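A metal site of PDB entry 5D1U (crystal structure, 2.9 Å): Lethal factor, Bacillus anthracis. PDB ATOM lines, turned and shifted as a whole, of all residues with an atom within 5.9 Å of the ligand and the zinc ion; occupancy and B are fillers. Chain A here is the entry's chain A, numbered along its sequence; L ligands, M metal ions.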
ATOM      1  N   ASP A  67     -19.738  14.975  15.573  1.00  0.00           N
ATOM      2  CA  ASP A  67     -18.313  15.304  15.545  1.00  0.00           C
ATOM      3  C   ASP A  67     -17.727  15.419  16.954  1.00  0.00           C
ATOM      4  O   ASP A  67     -16.747  14.757  17.269  1.00  0.00           O
ATOM      5  CB  ASP A  67     -18.075  16.601  14.781  1.00  0.00           C
ATOM      6  N   PHE A  68     -18.335  16.269  17.788  1.00  0.00           N
ATOM      7  CA  PHE A  68     -17.777  16.590  19.102  1.00  0.00           C
ATOM      8  C   PHE A  68     -18.379  15.797  20.265  1.00  0.00           C
ATOM      9  O   PHE A  68     -17.894  15.864  21.393  1.00  0.00           O
ATOM     10  CB  PHE A  68     -17.936  18.087  19.388  1.00  0.00           C
ATOM     11  N   VAL A 392     -11.918  24.201  21.424  1.00  0.00           N
ATOM     12  CA  VAL A 392     -11.943  22.851  20.923  1.00  0.00           C
ATOM     13  C   VAL A 392     -10.910  21.957  21.588  1.00  0.00           C
ATOM     14  O   VAL A 392      -9.800  22.420  21.849  1.00  0.00           O
ATOM     15  CB  VAL A 392     -11.699  22.859  19.396  1.00  0.00           C
ATOM     16  CG1 VAL A 392     -11.266  21.496  18.885  1.00  0.00           C
ATOM     17  CG2 VAL A 392     -12.937  23.320  18.715  1.00  0.00           C
ATOM     18  N   HIS A 393     -11.291  20.713  21.882  1.00  0.00           N
ATOM     19  CA  HIS A 393     -10.343  19.644  22.242  1.00  0.00           C
ATOM     20  C   HIS A 393     -10.369  18.519  21.188  1.00  0.00           C
ATOM     21  O   HIS A 393     -11.448  18.190  20.693  1.00  0.00           O
ATOM     22  CB  HIS A 393     -10.672  19.074  23.611  1.00  0.00           C
ATOM     23  CG  HIS A 393      -9.846  17.881  23.986  1.00  0.00           C
ATOM     24  ND1 HIS A 393      -8.479  17.857  23.861  1.00  0.00           N
ATOM     25  CD2 HIS A 393     -10.204  16.666  24.470  1.00  0.00           C
ATOM     26  CE1 HIS A 393      -8.016  16.684  24.259  1.00  0.00           C
ATOM     27  NE2 HIS A 393      -9.039  15.941  24.626  1.00  0.00           N
ATOM     28  N   SER A 394      -9.210  17.924  20.875  1.00  0.00           N
ATOM     29  CA  SER A 394      -9.065  16.889  19.829  1.00  0.00           C
ATOM     30  C   SER A 394      -7.591  16.488  19.650  1.00  0.00           C
ATOM     31  O   SER A 394      -6.727  17.084  20.299  1.00  0.00           O
ATOM     32  CB  SER A 394      -9.633  17.366  18.499  1.00  0.00           C
ATOM     33  OG  SER A 394      -8.995  18.578  18.125  1.00  0.00           O
ATOM     34  N   LYS A 395      -7.286  15.531  18.765  1.00  0.00           N
ATOM     35  CA  LYS A 395      -5.924  14.983  18.624  1.00  0.00           C
ATOM     36  C   LYS A 395      -4.894  16.053  18.280  1.00  0.00           C
ATOM     37  O   LYS A 395      -3.742  15.994  18.712  1.00  0.00           O
ATOM     38  CB  LYS A 395      -5.882  13.871  17.566  1.00  0.00           C
ATOM     39  N   GLY A 396      -5.318  17.043  17.496  1.00  0.00           N
ATOM     40  CA  GLY A 396      -4.417  18.107  17.109  1.00  0.00           C
ATOM     41  C   GLY A 396      -5.139  19.349  16.625  1.00  0.00           C
ATOM     42  O   GLY A 396      -6.345  19.323  16.399  1.00  0.00           O
ATOM     43  N   LEU A 397      -4.404  20.448  16.464  1.00  0.00           N
ATOM     44  CA  LEU A 397      -5.036  21.714  16.114  1.00  0.00           C
ATOM     45  C   LEU A 397      -4.043  22.671  15.424  1.00  0.00           C
ATOM     46  O   LEU A 397      -2.834  22.613  15.674  1.00  0.00           O
ATOM     47  CB  LEU A 397      -5.613  22.377  17.384  1.00  0.00           C
ATOM     48  CG  LEU A 397      -6.830  23.290  17.250  1.00  0.00           C
ATOM     49  CD1 LEU A 397      -8.075  22.471  16.946  1.00  0.00           C
ATOM     50  CD2 LEU A 397      -7.023  24.093  18.497  1.00  0.00           C
ATOM     51  N   TYR A 398      -4.562  23.534  14.548  1.00  0.00           N
ATOM     52  CA  TYR A 398      -3.771  24.688  14.142  1.00  0.00           C
ATOM     53  C   TYR A 398      -4.489  25.973  14.522  1.00  0.00           C
ATOM     54  O   TYR A 398      -5.666  26.180  14.214  1.00  0.00           O
ATOM     55  CB  TYR A 398      -3.460  24.658  12.643  1.00  0.00           C
ATOM     56  CG  TYR A 398      -2.635  25.866  12.202  1.00  0.00           C
ATOM     57  CD1 TYR A 398      -1.299  25.989  12.560  1.00  0.00           C
ATOM     58  CD2 TYR A 398      -3.211  26.903  11.482  1.00  0.00           C
ATOM     59  CE1 TYR A 398      -0.561  27.073  12.205  1.00  0.00           C
ATOM     60  CE2 TYR A 398      -2.478  27.999  11.114  1.00  0.00           C
ATOM     61  CZ  TYR A 398      -1.152  28.083  11.471  1.00  0.00           C
ATOM     62  OH  TYR A 398      -0.386  29.180  11.102  1.00  0.00           O
ATOM     63  N   LYS A 412      -6.846   9.671  20.599  1.00  0.00           N
ATOM     64  CA  LYS A 412      -6.762   9.157  19.244  1.00  0.00           C
ATOM     65  C   LYS A 412      -7.777   9.847  18.342  1.00  0.00           C
ATOM     66  O   LYS A 412      -8.988   9.827  18.600  1.00  0.00           O
ATOM     67  CB  LYS A 412      -6.980   7.643  19.246  1.00  0.00           C
ATOM     68  CG  LYS A 412      -6.853   6.985  17.865  1.00  0.00           C
ATOM     69  CD  LYS A 412      -7.184   5.486  17.952  1.00  0.00           C
ATOM     70  CE  LYS A 412      -7.184   4.798  16.582  1.00  0.00           C
ATOM     71  NZ  LYS A 412      -7.963   3.509  16.593  1.00  0.00           N
ATOM     72  N   GLY A 413      -7.289  10.470  17.280  1.00  0.00           N
ATOM     73  CA  GLY A 413      -8.163  11.096  16.302  1.00  0.00           C
ATOM     74  C   GLY A 413      -8.856  10.073  15.419  1.00  0.00           C
ATOM     75  O   GLY A 413      -8.286   9.029  15.118  1.00  0.00           O
ATOM     76  N   VAL A 414     -10.093  10.359  15.011  1.00  0.00           N
ATOM     77  CA  VAL A 414     -10.809   9.413  14.172  1.00  0.00           C
ATOM     78  C   VAL A 414     -10.177   9.379  12.794  1.00  0.00           C
ATOM     79  O   VAL A 414     -10.018  10.423  12.163  1.00  0.00           O
ATOM     80  CB  VAL A 414     -12.317   9.749  14.046  1.00  0.00           C
ATOM     81  CG1 VAL A 414     -12.959   8.980  12.890  1.00  0.00           C
ATOM     82  CG2 VAL A 414     -13.046   9.459  15.348  1.00  0.00           C
ATOM     83  N   GLU A 415      -9.786   8.168  12.392  1.00  0.00           N
ATOM     84  CA  GLU A 415      -9.248   7.846  11.082  1.00  0.00           C
ATOM     85  C   GLU A 415      -7.747   8.189  11.021  1.00  0.00           C
ATOM     86  O   GLU A 415      -7.203   8.427   9.932  1.00  0.00           O
ATOM     87  CB  GLU A 415     -10.009   8.602  10.004  1.00  0.00           C
ATOM     88  CG  GLU A 415     -11.343   8.026   9.588  1.00  0.00           C
ATOM     89  CD  GLU A 415     -12.122   9.006   8.727  1.00  0.00           C
ATOM     90  OE1 GLU A 415     -11.679  10.177   8.615  1.00  0.00           O
ATOM     91  OE2 GLU A 415     -13.167   8.609   8.160  1.00  0.00           O
ATOM     92  N   LEU A 416      -7.069   8.186  12.158  1.00  0.00           N
ATOM     93  CA  LEU A 416      -5.631   8.399  12.126  1.00  0.00           C
ATOM     94  C   LEU A 416      -4.924   7.151  12.576  1.00  0.00           C
ATOM     95  O   LEU A 416      -5.265   6.636  13.631  1.00  0.00           O
ATOM     96  CB  LEU A 416      -5.250   9.574  13.009  1.00  0.00           C
ATOM     97  CG  LEU A 416      -5.530  10.946  12.393  1.00  0.00           C
ATOM     98  CD1 LEU A 416      -5.202  12.070  13.347  1.00  0.00           C
ATOM     99  CD2 LEU A 416      -4.742  11.076  11.110  1.00  0.00           C
ATOM    100  N   GLU A 421       0.734  10.998  11.903  1.00  0.00           N
ATOM    101  CA  GLU A 421      -0.097  11.412  10.787  1.00  0.00           C
ATOM    102  C   GLU A 421      -0.907  12.671  11.084  1.00  0.00           C
ATOM    103  O   GLU A 421      -1.077  13.528  10.212  1.00  0.00           O
ATOM    104  CB  GLU A 421      -1.023  10.267  10.356  1.00  0.00           C
ATOM    105  CG  GLU A 421      -0.540   9.598   9.073  1.00  0.00           C
ATOM    106  CD  GLU A 421      -1.160   8.246   8.817  1.00  0.00           C
ATOM    107  OE1 GLU A 421      -2.223   7.950   9.418  1.00  0.00           O
ATOM    108  OE2 GLU A 421      -0.578   7.485   8.005  1.00  0.00           O
ATOM    109  N   GLY A 422      -1.369  12.810  12.326  1.00  0.00           N
ATOM    110  CA  GLY A 422      -2.233  13.906  12.707  1.00  0.00           C
ATOM    111  C   GLY A 422      -1.511  15.221  12.650  1.00  0.00           C
ATOM    112  O   GLY A 422      -2.089  16.257  12.311  1.00  0.00           O
ATOM    113  N   PHE A 423      -0.229  15.183  12.969  1.00  0.00           N
ATOM    114  CA  PHE A 423       0.627  16.352  12.867  1.00  0.00           C
ATOM    115  C   PHE A 423       0.652  16.878  11.435  1.00  0.00           C
ATOM    116  O   PHE A 423       0.407  18.063  11.194  1.00  0.00           O
ATOM    117  CB  PHE A 423       2.045  16.038  13.331  1.00  0.00           C
ATOM    118  CG  PHE A 423       2.885  17.253  13.544  1.00  0.00           C
ATOM    119  CD1 PHE A 423       2.832  17.939  14.747  1.00  0.00           C
ATOM    120  CD2 PHE A 423       3.716  17.735  12.539  1.00  0.00           C
ATOM    121  CE1 PHE A 423       3.600  19.079  14.954  1.00  0.00           C
ATOM    122  CE2 PHE A 423       4.486  18.874  12.737  1.00  0.00           C
ATOM    123  CZ  PHE A 423       4.420  19.554  13.947  1.00  0.00           C
ATOM    124  N   HIS A 425      -1.382  16.480   9.109  1.00  0.00           N
ATOM    125  CA  HIS A 425      -2.656  17.142   8.897  1.00  0.00           C
ATOM    126  C   HIS A 425      -2.630  18.606   9.384  1.00  0.00           C
ATOM    127  O   HIS A 425      -3.149  19.493   8.703  1.00  0.00           O
ATOM    128  CB  HIS A 425      -3.804  16.390   9.573  1.00  0.00           C
ATOM    129  CG  HIS A 425      -5.115  17.107   9.525  1.00  0.00           C
ATOM    130  ND1 HIS A 425      -6.138  16.734   8.685  1.00  0.00           N
ATOM    131  CD2 HIS A 425      -5.569  18.192  10.204  1.00  0.00           C
ATOM    132  CE1 HIS A 425      -7.170  17.549   8.848  1.00  0.00           C
ATOM    133  NE2 HIS A 425      -6.851  18.439   9.766  1.00  0.00           N
ATOM    134  N   GLU A 426      -2.051  18.874  10.560  1.00  0.00           N
ATOM    135  CA  GLU A 426      -2.026  20.255  11.091  1.00  0.00           C
ATOM    136  C   GLU A 426      -1.071  21.162  10.332  1.00  0.00           C
ATOM    137  O   GLU A 426      -1.396  22.298  10.021  1.00  0.00           O
ATOM    138  CB  GLU A 426      -1.663  20.280  12.572  1.00  0.00           C
ATOM    139  CG  GLU A 426      -2.503  19.380  13.474  1.00  0.00           C
ATOM    140  CD  GLU A 426      -3.977  19.726  13.428  1.00  0.00           C
ATOM    141  OE1 GLU A 426      -4.795  18.812  13.645  1.00  0.00           O
ATOM    142  OE2 GLU A 426      -4.292  20.909  13.169  1.00  0.00           O
ATOM    143  N   HIS A 429      -2.613  22.582   7.618  1.00  0.00           N
ATOM    144  CA  HIS A 429      -3.305  23.843   7.913  1.00  0.00           C
ATOM    145  C   HIS A 429      -2.365  25.071   7.872  1.00  0.00           C
ATOM    146  O   HIS A 429      -2.782  26.161   7.457  1.00  0.00           O
ATOM    147  CB  HIS A 429      -3.973  23.772   9.286  1.00  0.00           C
ATOM    148  CG  HIS A 429      -5.227  22.965   9.319  1.00  0.00           C
ATOM    149  ND1 HIS A 429      -6.319  23.228   8.525  1.00  0.00           N
ATOM    150  CD2 HIS A 429      -5.587  21.916  10.107  1.00  0.00           C
ATOM    151  CE1 HIS A 429      -7.287  22.370   8.806  1.00  0.00           C
ATOM    152  NE2 HIS A 429      -6.869  21.562   9.759  1.00  0.00           N
ATOM    153  N   TYR A 467     -14.109  12.614   6.671  1.00  0.00           N
ATOM    154  CA  TYR A 467     -13.941  13.846   7.448  1.00  0.00           C
ATOM    155  C   TYR A 467     -13.534  15.021   6.565  1.00  0.00           C
ATOM    156  O   TYR A 467     -13.747  16.188   6.930  1.00  0.00           O
ATOM    157  CB  TYR A 467     -12.919  13.643   8.573  1.00  0.00           C
ATOM    158  CG  TYR A 467     -12.693  14.879   9.416  1.00  0.00           C
ATOM    159  CD1 TYR A 467     -13.765  15.536   9.996  1.00  0.00           C
ATOM    160  CD2 TYR A 467     -11.417  15.384   9.614  1.00  0.00           C
ATOM    161  CE1 TYR A 467     -13.584  16.673  10.748  1.00  0.00           C
ATOM    162  CE2 TYR A 467     -11.227  16.529  10.378  1.00  0.00           C
ATOM    163  CZ  TYR A 467     -12.309  17.168  10.936  1.00  0.00           C
ATOM    164  OH  TYR A 467     -12.152  18.311  11.703  1.00  0.00           O
ATOM    165  N   GLU A 474     -10.438  21.883   5.927  1.00  0.00           N
ATOM    166  CA  GLU A 474     -10.164  20.529   6.377  1.00  0.00           C
ATOM    167  C   GLU A 474      -9.918  19.627   5.197  1.00  0.00           C
ATOM    168  O   GLU A 474      -9.054  18.755   5.252  1.00  0.00           O
ATOM    169  CB  GLU A 474     -11.313  19.978   7.222  1.00  0.00           C
ATOM    170  CG  GLU A 474     -11.615  20.725   8.505  1.00  0.00           C
ATOM    171  CD  GLU A 474     -10.516  20.598   9.534  1.00  0.00           C
ATOM    172  OE1 GLU A 474     -10.213  19.465   9.932  1.00  0.00           O
ATOM    173  OE2 GLU A 474      -9.984  21.635   9.974  1.00  0.00           O
ATOM    174  N   ALA A 477      -6.526  20.064   4.252  1.00  0.00           N
ATOM    175  CA  ALA A 477      -5.611  19.479   5.238  1.00  0.00           C
ATOM    176  C   ALA A 477      -5.519  17.964   5.070  1.00  0.00           C
ATOM    177  O   ALA A 477      -4.421  17.410   4.957  1.00  0.00           O
ATOM    178  CB  ALA A 477      -6.043  19.812   6.646  1.00  0.00           C
ATOM    179  N   GLU A 478      -6.665  17.307   5.043  1.00  0.00           N
ATOM    180  CA  GLU A 478      -6.694  15.875   4.853  1.00  0.00           C
ATOM    181  C   GLU A 478      -6.025  15.469   3.526  1.00  0.00           C
ATOM    182  O   GLU A 478      -5.260  14.501   3.498  1.00  0.00           O
ATOM    183  CB  GLU A 478      -8.131  15.351   4.935  1.00  0.00           C
ATOM    184  CG  GLU A 478      -8.624  15.141   6.355  1.00  0.00           C
ATOM    185  CD  GLU A 478      -8.012  13.900   7.019  1.00  0.00           C
ATOM    186  OE1 GLU A 478      -8.770  12.975   7.406  1.00  0.00           O
ATOM    187  OE2 GLU A 478      -6.767  13.846   7.175  1.00  0.00           O
ATOM    188  N   ARG A 481      -2.515  15.665   3.998  1.00  0.00           N
ATOM    189  CA  ARG A 481      -2.072  14.555   4.832  1.00  0.00           C
ATOM    190  C   ARG A 481      -1.830  13.313   3.982  1.00  0.00           C
ATOM    191  O   ARG A 481      -0.721  12.773   3.964  1.00  0.00           O
ATOM    192  CB  ARG A 481      -3.100  14.255   5.917  1.00  0.00           C
ATOM    193  CG  ARG A 481      -2.714  13.115   6.820  1.00  0.00           C
ATOM    194  CD  ARG A 481      -3.712  12.900   7.919  1.00  0.00           C
ATOM    195  NE  ARG A 481      -4.993  12.375   7.432  1.00  0.00           N
ATOM    196  CZ  ARG A 481      -5.211  11.098   7.139  1.00  0.00           C
ATOM    197  NH1 ARG A 481      -4.244  10.187   7.251  1.00  0.00           N
ATOM    198  NH2 ARG A 481      -6.425  10.729   6.715  1.00  0.00           N
HETATM  199  C1  LIG L   1      -9.337  18.484  14.827  1.00  0.00           C
HETATM  200  C2  LIG L   1      -8.812  19.115  13.547  1.00  0.00           C
HETATM  201  C3  LIG L   1     -13.621  16.736  14.788  1.00  0.00           C
HETATM  202  O1  LIG L   1      -7.296  20.589  12.548  1.00  0.00           O
HETATM  203  N1  LIG L   1      -9.822  17.081  14.781  1.00  0.00           N
HETATM  204  C4  LIG L   1      -8.077  15.439  13.851  1.00  0.00           C
HETATM  205  C5  LIG L   1      -8.587  14.557  12.896  1.00  0.00           C
HETATM  206  C6  LIG L   1      -7.833  14.236  11.784  1.00  0.00           C
HETATM  207  C7  LIG L   1      -6.576  14.789  11.604  1.00  0.00           C
HETATM  208  C8  LIG L   1      -6.057  15.658  12.552  1.00  0.00           C
HETATM  209  C9  LIG L   1      -6.809  15.989  13.664  1.00  0.00           C
HETATM  210  C10 LIG L   1     -12.207  16.575  15.339  1.00  0.00           C
HETATM  211  C11 LIG L   1     -11.204  17.015  14.286  1.00  0.00           C
HETATM  212  C12 LIG L   1     -10.423  19.446  15.312  1.00  0.00           C
HETATM  213  N2  LIG L   1      -7.727  19.877  13.669  1.00  0.00           N
HETATM  214  O2  LIG L   1      -9.373  19.004  12.463  1.00  0.00           O
HETATM  215  S1  LIG L   1      -8.933  15.841  15.152  1.00  0.00           S
HETATM  216  O3  LIG L   1      -9.665  14.670  15.604  1.00  0.00           O
HETATM  217  O4  LIG L   1      -7.989  16.176  16.180  1.00  0.00           O
HETATM  218  F1  LIG L   1      -5.860  14.467  10.514  1.00  0.00           F
HETATM  219  C13 LIG L   1      -8.383  13.284  10.749  1.00  0.00           C
HETATM  220 ZN    ZN M   1      -7.900  20.068  10.755  1.00  0.00          ZN
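The backbone NH (N) of Lys 395 lies within hydrogen-bond range of an oxygen (O4) of the ligand (2.8 Å).
O2 of the ligand lies close to OH of Tyr 467 (3.0 Å).
The side-chain hydroxyl (OG) of Ser 394 lies close to an oxygen (O4) of the ligand (3.3 Å).
The side-chain carboxylate (OE1) of Glu 426 is in hydrogen-bond range of a nitrogen (N2) of the ligand, 3.1 Å away.
N of Gly 396 sits at hydrogen-bond distance from O4 of the ligand.
A nitrogen (N2) of the ligand is in hydrogen-bond range of the backbone carbonyl oxygen of Gly 396 (3.1 Å).
Residues that only touch the ligand: Gly 413 (3.9 Å), Val 414 (3.6 Å), Leu 416 (3.5 Å), Glu 478 (3.4 Å) and Arg 481 (3.7 Å).
Hydrophobic or aromatic side chains within 4 Å of the ligand: Leu 416, His 425, His 429 and Tyr 467.
Within 4 Å of the ligand: Ser 394, Lys 395, Gly 396, Gly 413, Val 414, Leu 416, His 425, Glu 426, His 429, Tyr 467, Glu 474, Glu 478 and Arg 481.
Along chain A the residues within 4 Å of the ligand span positions 394 to 481.
The zinc ion is bound by an oxygen (O1) of the ligand (2.0 Å), a ring nitrogen (NE2) of His 429 (2.1 Å), a ring nitrogen (NE2) of His 425 (2.2 Å), an oxygen (O2) of the ligand (2.5 Å) and the side-chain carboxylate of Glu 474 (2.5 Å).
The zinc ion has five donor atoms within binding distance.
Slightly farther from the zinc ion lies OE2 of Glu 474 (2.7 Å).
Three residues have an atom within 4 Å of the zinc ion: His 425, His 429 and Glu 474.
The nearest printed residue that does not touch the zinc ion is Glu 426 (4.4 Å).
A ring nitrogen (ND1) of His 425 lies within hydrogen-bond range of the side-chain carboxylate of Glu 478, at 3.3 Å.
The side-chain hydroxyl (OH) of Tyr 467 sits close to the side-chain carboxylate (OE1) of Glu 474.
The backbone carbonyl oxygen of Gly 396 is in hydrogen-bond range of the side-chain hydroxyl of Ser 394 (3.2 Å).
The backbone NH of Leu 397 sits close to the side-chain carboxylate of Glu 426, 3.3 Å away.
N of Tyr 398 sits at hydrogen-bond distance from OE2 of Glu 426.
The side-chain carboxylate (OE2) of Glu 478 lies within salt-bridge range of the guanidinium group (NH2) of Arg 481.
The guanidinium group of Arg 481 is in salt-bridge range of the side-chain carboxylate of Glu 421.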
